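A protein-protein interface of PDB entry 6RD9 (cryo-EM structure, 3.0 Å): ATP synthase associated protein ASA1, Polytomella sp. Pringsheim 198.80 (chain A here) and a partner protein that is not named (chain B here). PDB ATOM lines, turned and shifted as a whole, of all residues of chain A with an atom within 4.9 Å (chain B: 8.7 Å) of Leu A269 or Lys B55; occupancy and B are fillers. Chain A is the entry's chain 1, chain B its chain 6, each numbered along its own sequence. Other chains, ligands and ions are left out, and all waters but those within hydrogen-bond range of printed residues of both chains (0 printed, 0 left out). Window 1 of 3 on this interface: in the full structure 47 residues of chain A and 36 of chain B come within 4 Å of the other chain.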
ATOM      1  N   ALA A 265      -3.757 -23.483  -9.274  1.00  0.00           N
ATOM      2  CA  ALA A 265      -3.030 -22.303  -8.844  1.00  0.00           C
ATOM      3  C   ALA A 265      -3.923 -21.084  -8.862  1.00  0.00           C
ATOM      4  O   ALA A 265      -3.871 -20.272  -7.946  1.00  0.00           O
ATOM      5  CB  ALA A 265      -1.818 -22.070  -9.724  1.00  0.00           C
ATOM      6  N   LYS A 266      -4.766 -20.951  -9.879  1.00  0.00           N
ATOM      7  CA  LYS A 266      -5.669 -19.814  -9.940  1.00  0.00           C
ATOM      8  C   LYS A 266      -6.769 -19.911  -8.906  1.00  0.00           C
ATOM      9  O   LYS A 266      -7.221 -18.896  -8.388  1.00  0.00           O
ATOM     10  CB  LYS A 266      -6.286 -19.713 -11.319  1.00  0.00           C
ATOM     11  CG  LYS A 266      -5.322 -19.846 -12.418  1.00  0.00           C
ATOM     12  CD  LYS A 266      -6.045 -20.154 -13.661  1.00  0.00           C
ATOM     13  CE  LYS A 266      -5.104 -20.490 -14.756  1.00  0.00           C
ATOM     14  NZ  LYS A 266      -5.843 -20.957 -15.932  1.00  0.00           N
ATOM     15  N   ARG A 267      -7.216 -21.106  -8.599  1.00  0.00           N
ATOM     16  CA  ARG A 267      -8.339 -21.260  -7.702  1.00  0.00           C
ATOM     17  C   ARG A 267      -7.928 -21.086  -6.265  1.00  0.00           C
ATOM     18  O   ARG A 267      -8.780 -20.840  -5.421  1.00  0.00           O
ATOM     19  CB  ARG A 267      -8.976 -22.630  -7.880  1.00  0.00           C
ATOM     20  CG  ARG A 267     -10.080 -22.702  -8.876  1.00  0.00           C
ATOM     21  CD  ARG A 267      -9.547 -22.645 -10.238  1.00  0.00           C
ATOM     22  NE  ARG A 267     -10.515 -22.975 -11.242  1.00  0.00           N
ATOM     23  CZ  ARG A 267     -10.312 -22.792 -12.527  1.00  0.00           C
ATOM     24  NH1 ARG A 267      -9.180 -22.277 -12.936  1.00  0.00           N
ATOM     25  NH2 ARG A 267     -11.246 -23.099 -13.394  1.00  0.00           N
ATOM     26  N   LEU A 268      -6.648 -21.228  -5.970  1.00  0.00           N
ATOM     27  CA  LEU A 268      -6.124 -21.041  -4.637  1.00  0.00           C
ATOM     28  C   LEU A 268      -5.375 -19.738  -4.479  1.00  0.00           C
ATOM     29  O   LEU A 268      -4.934 -19.429  -3.375  1.00  0.00           O
ATOM     30  CB  LEU A 268      -5.207 -22.206  -4.259  1.00  0.00           C
ATOM     31  CG  LEU A 268      -5.883 -23.565  -4.138  1.00  0.00           C
ATOM     32  CD1 LEU A 268      -4.856 -24.619  -4.177  1.00  0.00           C
ATOM     33  CD2 LEU A 268      -6.616 -23.673  -2.857  1.00  0.00           C
ATOM     34  N   LEU A 269      -5.191 -18.982  -5.548  1.00  0.00           N
ATOM     35  CA  LEU A 269      -4.747 -17.607  -5.405  1.00  0.00           C
ATOM     36  C   LEU A 269      -5.932 -16.698  -5.159  1.00  0.00           C
ATOM     37  O   LEU A 269      -5.860 -15.782  -4.337  1.00  0.00           O
ATOM     38  CB  LEU A 269      -3.994 -17.165  -6.650  1.00  0.00           C
ATOM     39  CG  LEU A 269      -2.540 -17.581  -6.758  1.00  0.00           C
ATOM     40  CD1 LEU A 269      -1.997 -17.157  -8.077  1.00  0.00           C
ATOM     41  CD2 LEU A 269      -1.789 -16.968  -5.677  1.00  0.00           C
ATOM     42  N   VAL A 270      -7.030 -16.944  -5.863  1.00  0.00           N
ATOM     43  CA  VAL A 270      -8.257 -16.203  -5.625  1.00  0.00           C
ATOM     44  C   VAL A 270      -8.908 -16.664  -4.336  1.00  0.00           C
ATOM     45  O   VAL A 270      -9.219 -15.860  -3.455  1.00  0.00           O
ATOM     46  CB  VAL A 270      -9.204 -16.367  -6.818  1.00  0.00           C
ATOM     47  CG1 VAL A 270     -10.540 -15.859  -6.472  1.00  0.00           C
ATOM     48  CG2 VAL A 270      -8.669 -15.644  -7.999  1.00  0.00           C
ATOM     49  N   SER A 271      -9.104 -17.966  -4.194  1.00  0.00           N
ATOM     50  CA  SER A 271      -9.947 -18.535  -3.155  1.00  0.00           C
ATOM     51  C   SER A 271      -9.185 -19.591  -2.373  1.00  0.00           C
ATOM     52  O   SER A 271      -9.450 -20.786  -2.532  1.00  0.00           O
ATOM     53  CB  SER A 271     -11.191 -19.149  -3.780  1.00  0.00           C
ATOM     54  OG  SER A 271     -11.882 -19.911  -2.833  1.00  0.00           O
ATOM     55  N   PRO A 272      -8.275 -19.195  -1.481  1.00  0.00           N
ATOM     56  CA  PRO A 272      -7.394 -20.181  -0.850  1.00  0.00           C
ATOM     57  C   PRO A 272      -8.057 -21.032   0.199  1.00  0.00           C
ATOM     58  O   PRO A 272      -7.430 -21.972   0.683  1.00  0.00           O
ATOM     59  CB  PRO A 272      -6.308 -19.315  -0.228  1.00  0.00           C
ATOM     60  CG  PRO A 272      -6.960 -18.083   0.049  1.00  0.00           C
ATOM     61  CD  PRO A 272      -7.930 -17.839  -1.053  1.00  0.00           C
ATOM     62  N   GLU A 352      -2.372 -18.512   3.380  1.00  0.00           N
ATOM     63  CA  GLU A 352      -1.986 -17.337   2.612  1.00  0.00           C
ATOM     64  C   GLU A 352      -0.707 -17.563   1.831  1.00  0.00           C
ATOM     65  O   GLU A 352      -0.359 -16.729   0.992  1.00  0.00           O
ATOM     66  CB  GLU A 352      -1.820 -16.103   3.501  1.00  0.00           C
ATOM     67  CG  GLU A 352      -3.091 -15.622   4.176  1.00  0.00           C
ATOM     68  CD  GLU A 352      -4.257 -15.419   3.215  1.00  0.00           C
ATOM     69  OE1 GLU A 352      -5.214 -16.218   3.265  1.00  0.00           O
ATOM     70  OE2 GLU A 352      -4.231 -14.457   2.423  1.00  0.00           O
ATOM     71  N   PRO A 354       0.301 -19.619  -1.079  1.00  0.00           N
ATOM     72  CA  PRO A 354      -0.403 -20.432  -2.070  1.00  0.00           C
ATOM     73  C   PRO A 354       0.310 -21.720  -2.422  1.00  0.00           C
ATOM     74  O   PRO A 354      -0.305 -22.587  -3.044  1.00  0.00           O
ATOM     75  CB  PRO A 354      -0.511 -19.497  -3.273  1.00  0.00           C
ATOM     76  CG  PRO A 354       0.551 -18.532  -3.088  1.00  0.00           C
ATOM     77  CD  PRO A 354       0.812 -18.371  -1.652  1.00  0.00           C
ATOM     78  N   SER B  31      -8.107  -8.133 -11.653  1.00  0.00           N
ATOM     79  CA  SER B  31      -6.938  -8.821 -11.156  1.00  0.00           C
ATOM     80  C   SER B  31      -7.029 -10.315 -11.302  1.00  0.00           C
ATOM     81  O   SER B  31      -6.019 -10.993 -11.161  1.00  0.00           O
ATOM     82  CB  SER B  31      -6.727  -8.497  -9.697  1.00  0.00           C
ATOM     83  OG  SER B  31      -7.734  -9.085  -8.919  1.00  0.00           O
ATOM     84  N   VAL B  32      -8.208 -10.854 -11.547  1.00  0.00           N
ATOM     85  CA  VAL B  32      -8.304 -12.281 -11.789  1.00  0.00           C
ATOM     86  C   VAL B  32      -7.834 -12.609 -13.193  1.00  0.00           C
ATOM     87  O   VAL B  32      -7.119 -13.587 -13.398  1.00  0.00           O
ATOM     88  CB  VAL B  32      -9.733 -12.753 -11.514  1.00  0.00           C
ATOM     89  CG1 VAL B  32      -9.869 -14.178 -11.817  1.00  0.00           C
ATOM     90  CG2 VAL B  32     -10.017 -12.558 -10.085  1.00  0.00           C
ATOM     91  N   GLY B  34      -5.593 -10.882 -14.504  1.00  0.00           N
ATOM     92  CA  GLY B  34      -4.167 -10.762 -14.324  1.00  0.00           C
ATOM     93  C   GLY B  34      -3.558 -11.973 -13.665  1.00  0.00           C
ATOM     94  O   GLY B  34      -2.395 -12.279 -13.898  1.00  0.00           O
ATOM     95  N   ILE B  35      -4.317 -12.662 -12.818  1.00  0.00           N
ATOM     96  CA  ILE B  35      -3.846 -13.906 -12.224  1.00  0.00           C
ATOM     97  C   ILE B  35      -3.818 -14.999 -13.271  1.00  0.00           C
ATOM     98  O   ILE B  35      -2.846 -15.746 -13.376  1.00  0.00           O
ATOM     99  CB  ILE B  35      -4.737 -14.293 -11.030  1.00  0.00           C
ATOM    100  CG1 ILE B  35      -4.319 -13.538  -9.788  1.00  0.00           C
ATOM    101  CG2 ILE B  35      -4.670 -15.751 -10.721  1.00  0.00           C
ATOM    102  CD1 ILE B  35      -5.209 -13.779  -8.616  1.00  0.00           C
ATOM    103  N   ILE B  36      -4.879 -15.094 -14.067  1.00  0.00           N
ATOM    104  CA  ILE B  36      -4.995 -16.118 -15.094  1.00  0.00           C
ATOM    105  C   ILE B  36      -3.913 -15.947 -16.142  1.00  0.00           C
ATOM    106  O   ILE B  36      -3.313 -16.925 -16.583  1.00  0.00           O
ATOM    107  CB  ILE B  36      -6.402 -16.066 -15.709  1.00  0.00           C
ATOM    108  CG1 ILE B  36      -7.426 -16.579 -14.716  1.00  0.00           C
ATOM    109  CG2 ILE B  36      -6.485 -16.848 -16.971  1.00  0.00           C
ATOM    110  CD1 ILE B  36      -8.797 -16.481 -15.200  1.00  0.00           C
ATOM    111  N   SER B  38      -0.905 -14.348 -15.688  1.00  0.00           N
ATOM    112  CA  SER B  38       0.396 -14.567 -15.073  1.00  0.00           C
ATOM    113  C   SER B  38       0.656 -16.012 -14.703  1.00  0.00           C
ATOM    114  O   SER B  38       1.812 -16.386 -14.529  1.00  0.00           O
ATOM    115  CB  SER B  38       0.533 -13.728 -13.817  1.00  0.00           C
ATOM    116  OG  SER B  38       0.644 -12.361 -14.137  1.00  0.00           O
ATOM    117  N   VAL B  39      -0.378 -16.819 -14.530  1.00  0.00           N
ATOM    118  CA  VAL B  39      -0.178 -18.233 -14.259  1.00  0.00           C
ATOM    119  C   VAL B  39      -0.089 -19.017 -15.563  1.00  0.00           C
ATOM    120  O   VAL B  39       0.659 -19.989 -15.650  1.00  0.00           O
ATOM    121  CB  VAL B  39      -1.298 -18.732 -13.326  1.00  0.00           C
ATOM    122  CG1 VAL B  39      -1.341 -20.197 -13.213  1.00  0.00           C
ATOM    123  CG2 VAL B  39      -1.088 -18.194 -11.956  1.00  0.00           C
ATOM    124  N   LEU B  47       6.520 -22.396 -11.502  1.00  0.00           N
ATOM    125  CA  LEU B  47       5.145 -22.111 -11.120  1.00  0.00           C
ATOM    126  C   LEU B  47       5.046 -21.909  -9.625  1.00  0.00           C
ATOM    127  O   LEU B  47       4.520 -20.900  -9.161  1.00  0.00           O
ATOM    128  CB  LEU B  47       4.216 -23.236 -11.553  1.00  0.00           C
ATOM    129  CG  LEU B  47       2.823 -23.147 -10.933  1.00  0.00           C
ATOM    130  CD1 LEU B  47       2.070 -22.015 -11.544  1.00  0.00           C
ATOM    131  CD2 LEU B  47       2.067 -24.410 -11.118  1.00  0.00           C
ATOM    132  N   SER B  49       7.246 -21.187  -7.456  1.00  0.00           N
ATOM    133  CA  SER B  49       7.967 -20.038  -6.938  1.00  0.00           C
ATOM    134  C   SER B  49       7.270 -18.737  -7.274  1.00  0.00           C
ATOM    135  O   SER B  49       7.365 -17.780  -6.506  1.00  0.00           O
ATOM    136  CB  SER B  49       9.384 -20.005  -7.493  1.00  0.00           C
ATOM    137  OG  SER B  49       9.401 -19.424  -8.782  1.00  0.00           O
ATOM    138  N   SER B  50       6.560 -18.687  -8.391  1.00  0.00           N
ATOM    139  CA  SER B  50       5.927 -17.455  -8.819  1.00  0.00           C
ATOM    140  C   SER B  50       4.640 -17.168  -8.082  1.00  0.00           C
ATOM    141  O   SER B  50       4.067 -16.100  -8.282  1.00  0.00           O
ATOM    142  CB  SER B  50       5.621 -17.508 -10.309  1.00  0.00           C
ATOM    143  OG  SER B  50       6.805 -17.638 -11.059  1.00  0.00           O
ATOM    144  N   LEU B  51       4.161 -18.078  -7.250  1.00  0.00           N
ATOM    145  CA  LEU B  51       2.811 -17.932  -6.745  1.00  0.00           C
ATOM    146  C   LEU B  51       2.690 -16.880  -5.664  1.00  0.00           C
ATOM    147  O   LEU B  51       1.577 -16.453  -5.382  1.00  0.00           O
ATOM    148  CB  LEU B  51       2.295 -19.270  -6.232  1.00  0.00           C
ATOM    149  CG  LEU B  51       1.879 -20.289  -7.286  1.00  0.00           C
ATOM    150  CD1 LEU B  51       1.047 -21.347  -6.658  1.00  0.00           C
ATOM    151  CD2 LEU B  51       1.156 -19.651  -8.435  1.00  0.00           C
ATOM    152  N   LYS B  52       3.789 -16.429  -5.072  1.00  0.00           N
ATOM    153  CA  LYS B  52       3.709 -15.337  -4.113  1.00  0.00           C
ATOM    154  C   LYS B  52       3.873 -13.973  -4.748  1.00  0.00           C
ATOM    155  O   LYS B  52       3.569 -12.973  -4.103  1.00  0.00           O
ATOM    156  CB  LYS B  52       4.749 -15.497  -3.016  1.00  0.00           C
ATOM    157  CG  LYS B  52       4.654 -16.809  -2.304  1.00  0.00           C
ATOM    158  CD  LYS B  52       5.186 -16.732  -0.894  1.00  0.00           C
ATOM    159  CE  LYS B  52       4.184 -16.093   0.033  1.00  0.00           C
ATOM    160  NZ  LYS B  52       4.535 -16.353   1.452  1.00  0.00           N
ATOM    161  N   THR B  53       4.361 -13.896  -5.977  1.00  0.00           N
ATOM    162  CA  THR B  53       4.421 -12.626  -6.671  1.00  0.00           C
ATOM    163  C   THR B  53       3.258 -12.433  -7.619  1.00  0.00           C
ATOM    164  O   THR B  53       3.070 -11.327  -8.124  1.00  0.00           O
ATOM    165  CB  THR B  53       5.725 -12.496  -7.456  1.00  0.00           C
ATOM    166  OG1 THR B  53       5.585 -13.129  -8.726  1.00  0.00           O
ATOM    167  CG2 THR B  53       6.845 -13.167  -6.703  1.00  0.00           C
ATOM    168  N   ILE B  54       2.507 -13.491  -7.902  1.00  0.00           N
ATOM    169  CA  ILE B  54       1.220 -13.348  -8.559  1.00  0.00           C
ATOM    170  C   ILE B  54       0.145 -13.105  -7.515  1.00  0.00           C
ATOM    171  O   ILE B  54      -0.861 -12.455  -7.796  1.00  0.00           O
ATOM    172  CB  ILE B  54       0.939 -14.589  -9.423  1.00  0.00           C
ATOM    173  CG1 ILE B  54       2.063 -14.795 -10.415  1.00  0.00           C
ATOM    174  CG2 ILE B  54      -0.290 -14.430 -10.238  1.00  0.00           C
ATOM    175  CD1 ILE B  54       1.983 -16.092 -11.124  1.00  0.00           C
ATOM    176  N   LYS B  55       0.354 -13.591  -6.297  1.00  0.00           N
ATOM    177  CA  LYS B  55      -0.552 -13.288  -5.201  1.00  0.00           C
ATOM    178  C   LYS B  55      -0.510 -11.815  -4.854  1.00  0.00           C
ATOM    179  O   LYS B  55      -1.550 -11.193  -4.633  1.00  0.00           O
ATOM    180  CB  LYS B  55      -0.179 -14.115  -3.981  1.00  0.00           C
ATOM    181  CG  LYS B  55      -0.987 -13.874  -2.755  1.00  0.00           C
ATOM    182  CD  LYS B  55      -2.252 -14.663  -2.790  1.00  0.00           C
ATOM    183  CE  LYS B  55      -2.901 -14.695  -1.440  1.00  0.00           C
ATOM    184  NZ  LYS B  55      -4.220 -15.367  -1.501  1.00  0.00           N
ATOM    185  N   ALA B  56       0.683 -11.239  -4.814  1.00  0.00           N
ATOM    186  CA  ALA B  56       0.861  -9.857  -4.416  1.00  0.00           C
ATOM    187  C   ALA B  56       0.674  -8.881  -5.559  1.00  0.00           C
ATOM    188  O   ALA B  56       0.527  -7.690  -5.308  1.00  0.00           O
ATOM    189  CB  ALA B  56       2.241  -9.671  -3.811  1.00  0.00           C
ATOM    190  N   GLN B  57       0.706  -9.339  -6.800  1.00  0.00           N
ATOM    191  CA  GLN B  57       0.370  -8.464  -7.908  1.00  0.00           C
ATOM    192  C   GLN B  57      -1.123  -8.266  -8.046  1.00  0.00           C
ATOM    193  O   GLN B  57      -1.553  -7.353  -8.752  1.00  0.00           O
ATOM    194  CB  GLN B  57       0.907  -9.029  -9.212  1.00  0.00           C
ATOM    195  CG  GLN B  57       2.218  -8.463  -9.643  1.00  0.00           C
ATOM    196  CD  GLN B  57       2.800  -9.208 -10.820  1.00  0.00           C
ATOM    197  OE1 GLN B  57       2.347 -10.295 -11.164  1.00  0.00           O
ATOM    198  NE2 GLN B  57       3.817  -8.630 -11.443  1.00  0.00           N
ATOM    199  N   ALA B  58      -1.917  -9.118  -7.412  1.00  0.00           N
ATOM    200  CA  ALA B  58      -3.365  -9.051  -7.479  1.00  0.00           C
ATOM    201  C   ALA B  58      -3.989  -8.795  -6.125  1.00  0.00           C
ATOM    202  O   ALA B  58      -5.203  -8.926  -5.985  1.00  0.00           O
ATOM    203  CB  ALA B  58      -3.926 -10.338  -8.052  1.00  0.00           C
ATOM    204  N   ALA B  59      -3.188  -8.475  -5.125  1.00  0.00           N
ATOM    205  CA  ALA B  59      -3.716  -7.996  -3.874  1.00  0.00           C
ATOM    206  C   ALA B  59      -4.289  -6.603  -4.085  1.00  0.00           C
ATOM    207  O   ALA B  59      -3.823  -5.870  -4.953  1.00  0.00           O
ATOM    208  CB  ALA B  59      -2.620  -7.962  -2.826  1.00  0.00           C
ATOM    209  N   PRO B  60      -5.319  -6.221  -3.337  1.00  0.00           N
ATOM    210  CA  PRO B  60      -5.860  -4.875  -3.487  1.00  0.00           C
ATOM    211  C   PRO B  60      -4.944  -3.848  -2.858  1.00  0.00           C
ATOM    212  O   PRO B  60      -4.149  -4.145  -1.969  1.00  0.00           O
ATOM    213  CB  PRO B  60      -7.190  -4.955  -2.756  1.00  0.00           C
ATOM    214  CG  PRO B  60      -6.995  -5.988  -1.790  1.00  0.00           C
ATOM    215  CD  PRO B  60      -6.139  -7.008  -2.407  1.00  0.00           C
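Printed residues of chain B that touch a printed residue of chain A: Val B32, Ile B35, Ile B36, Val B39, Leu B51, Ile B54 and Lys B55.
Printed residues of chain A that touch a printed residue of chain B: Ala A265, Lys A266, Leu A269, Val A270 and Pro A354.
Among the printed residues, 8 pairs touch across the chains.
Among the printed residues, no Asp or Glu carboxylate lies within 4 Å of a Lys or Arg side-chain nitrogen of the other chain.
Printed residues of chain B within 4 Å of Leu A269: Leu B51, Ile B54 and Lys B55.
Lys B55 touches just one residue of chain A: Leu A269 (3.3 Å).
Of the printed residues of chain B, Ala A265 touches Val B39 (3.99 Å).
Printed residues of chain B within 4 Å of Lys A266: Ile B36.
Printed residues of chain A within 4 Å of Val B39: Ala A265 (3.99 Å).
Printed residues of chain B within 4 Å of Val A270: Val B32 (3.96 Å) and Ile B35 (3.98 Å).
Ser A271 touches none of the printed residues of chain B.
The side-chain amino group of Lys B55 is in hydrogen-bond range of the backbone carbonyl oxygen of Leu A269 (3.3 Å).
Among the printed residues, merely in contact across the chains: Ala A265 with Val B39 (3.99 Å), Lys A266 with Ile B36 (3.98 Å), Leu A269 with Leu B51 (3.4 Å), Leu A269 with Ile B54 (3.9 Å), Val A270 with Val B32 (3.96 Å), Val A270 with Ile B35 (3.98 Å) and Pro A354 with Leu B51 (3.3 Å).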
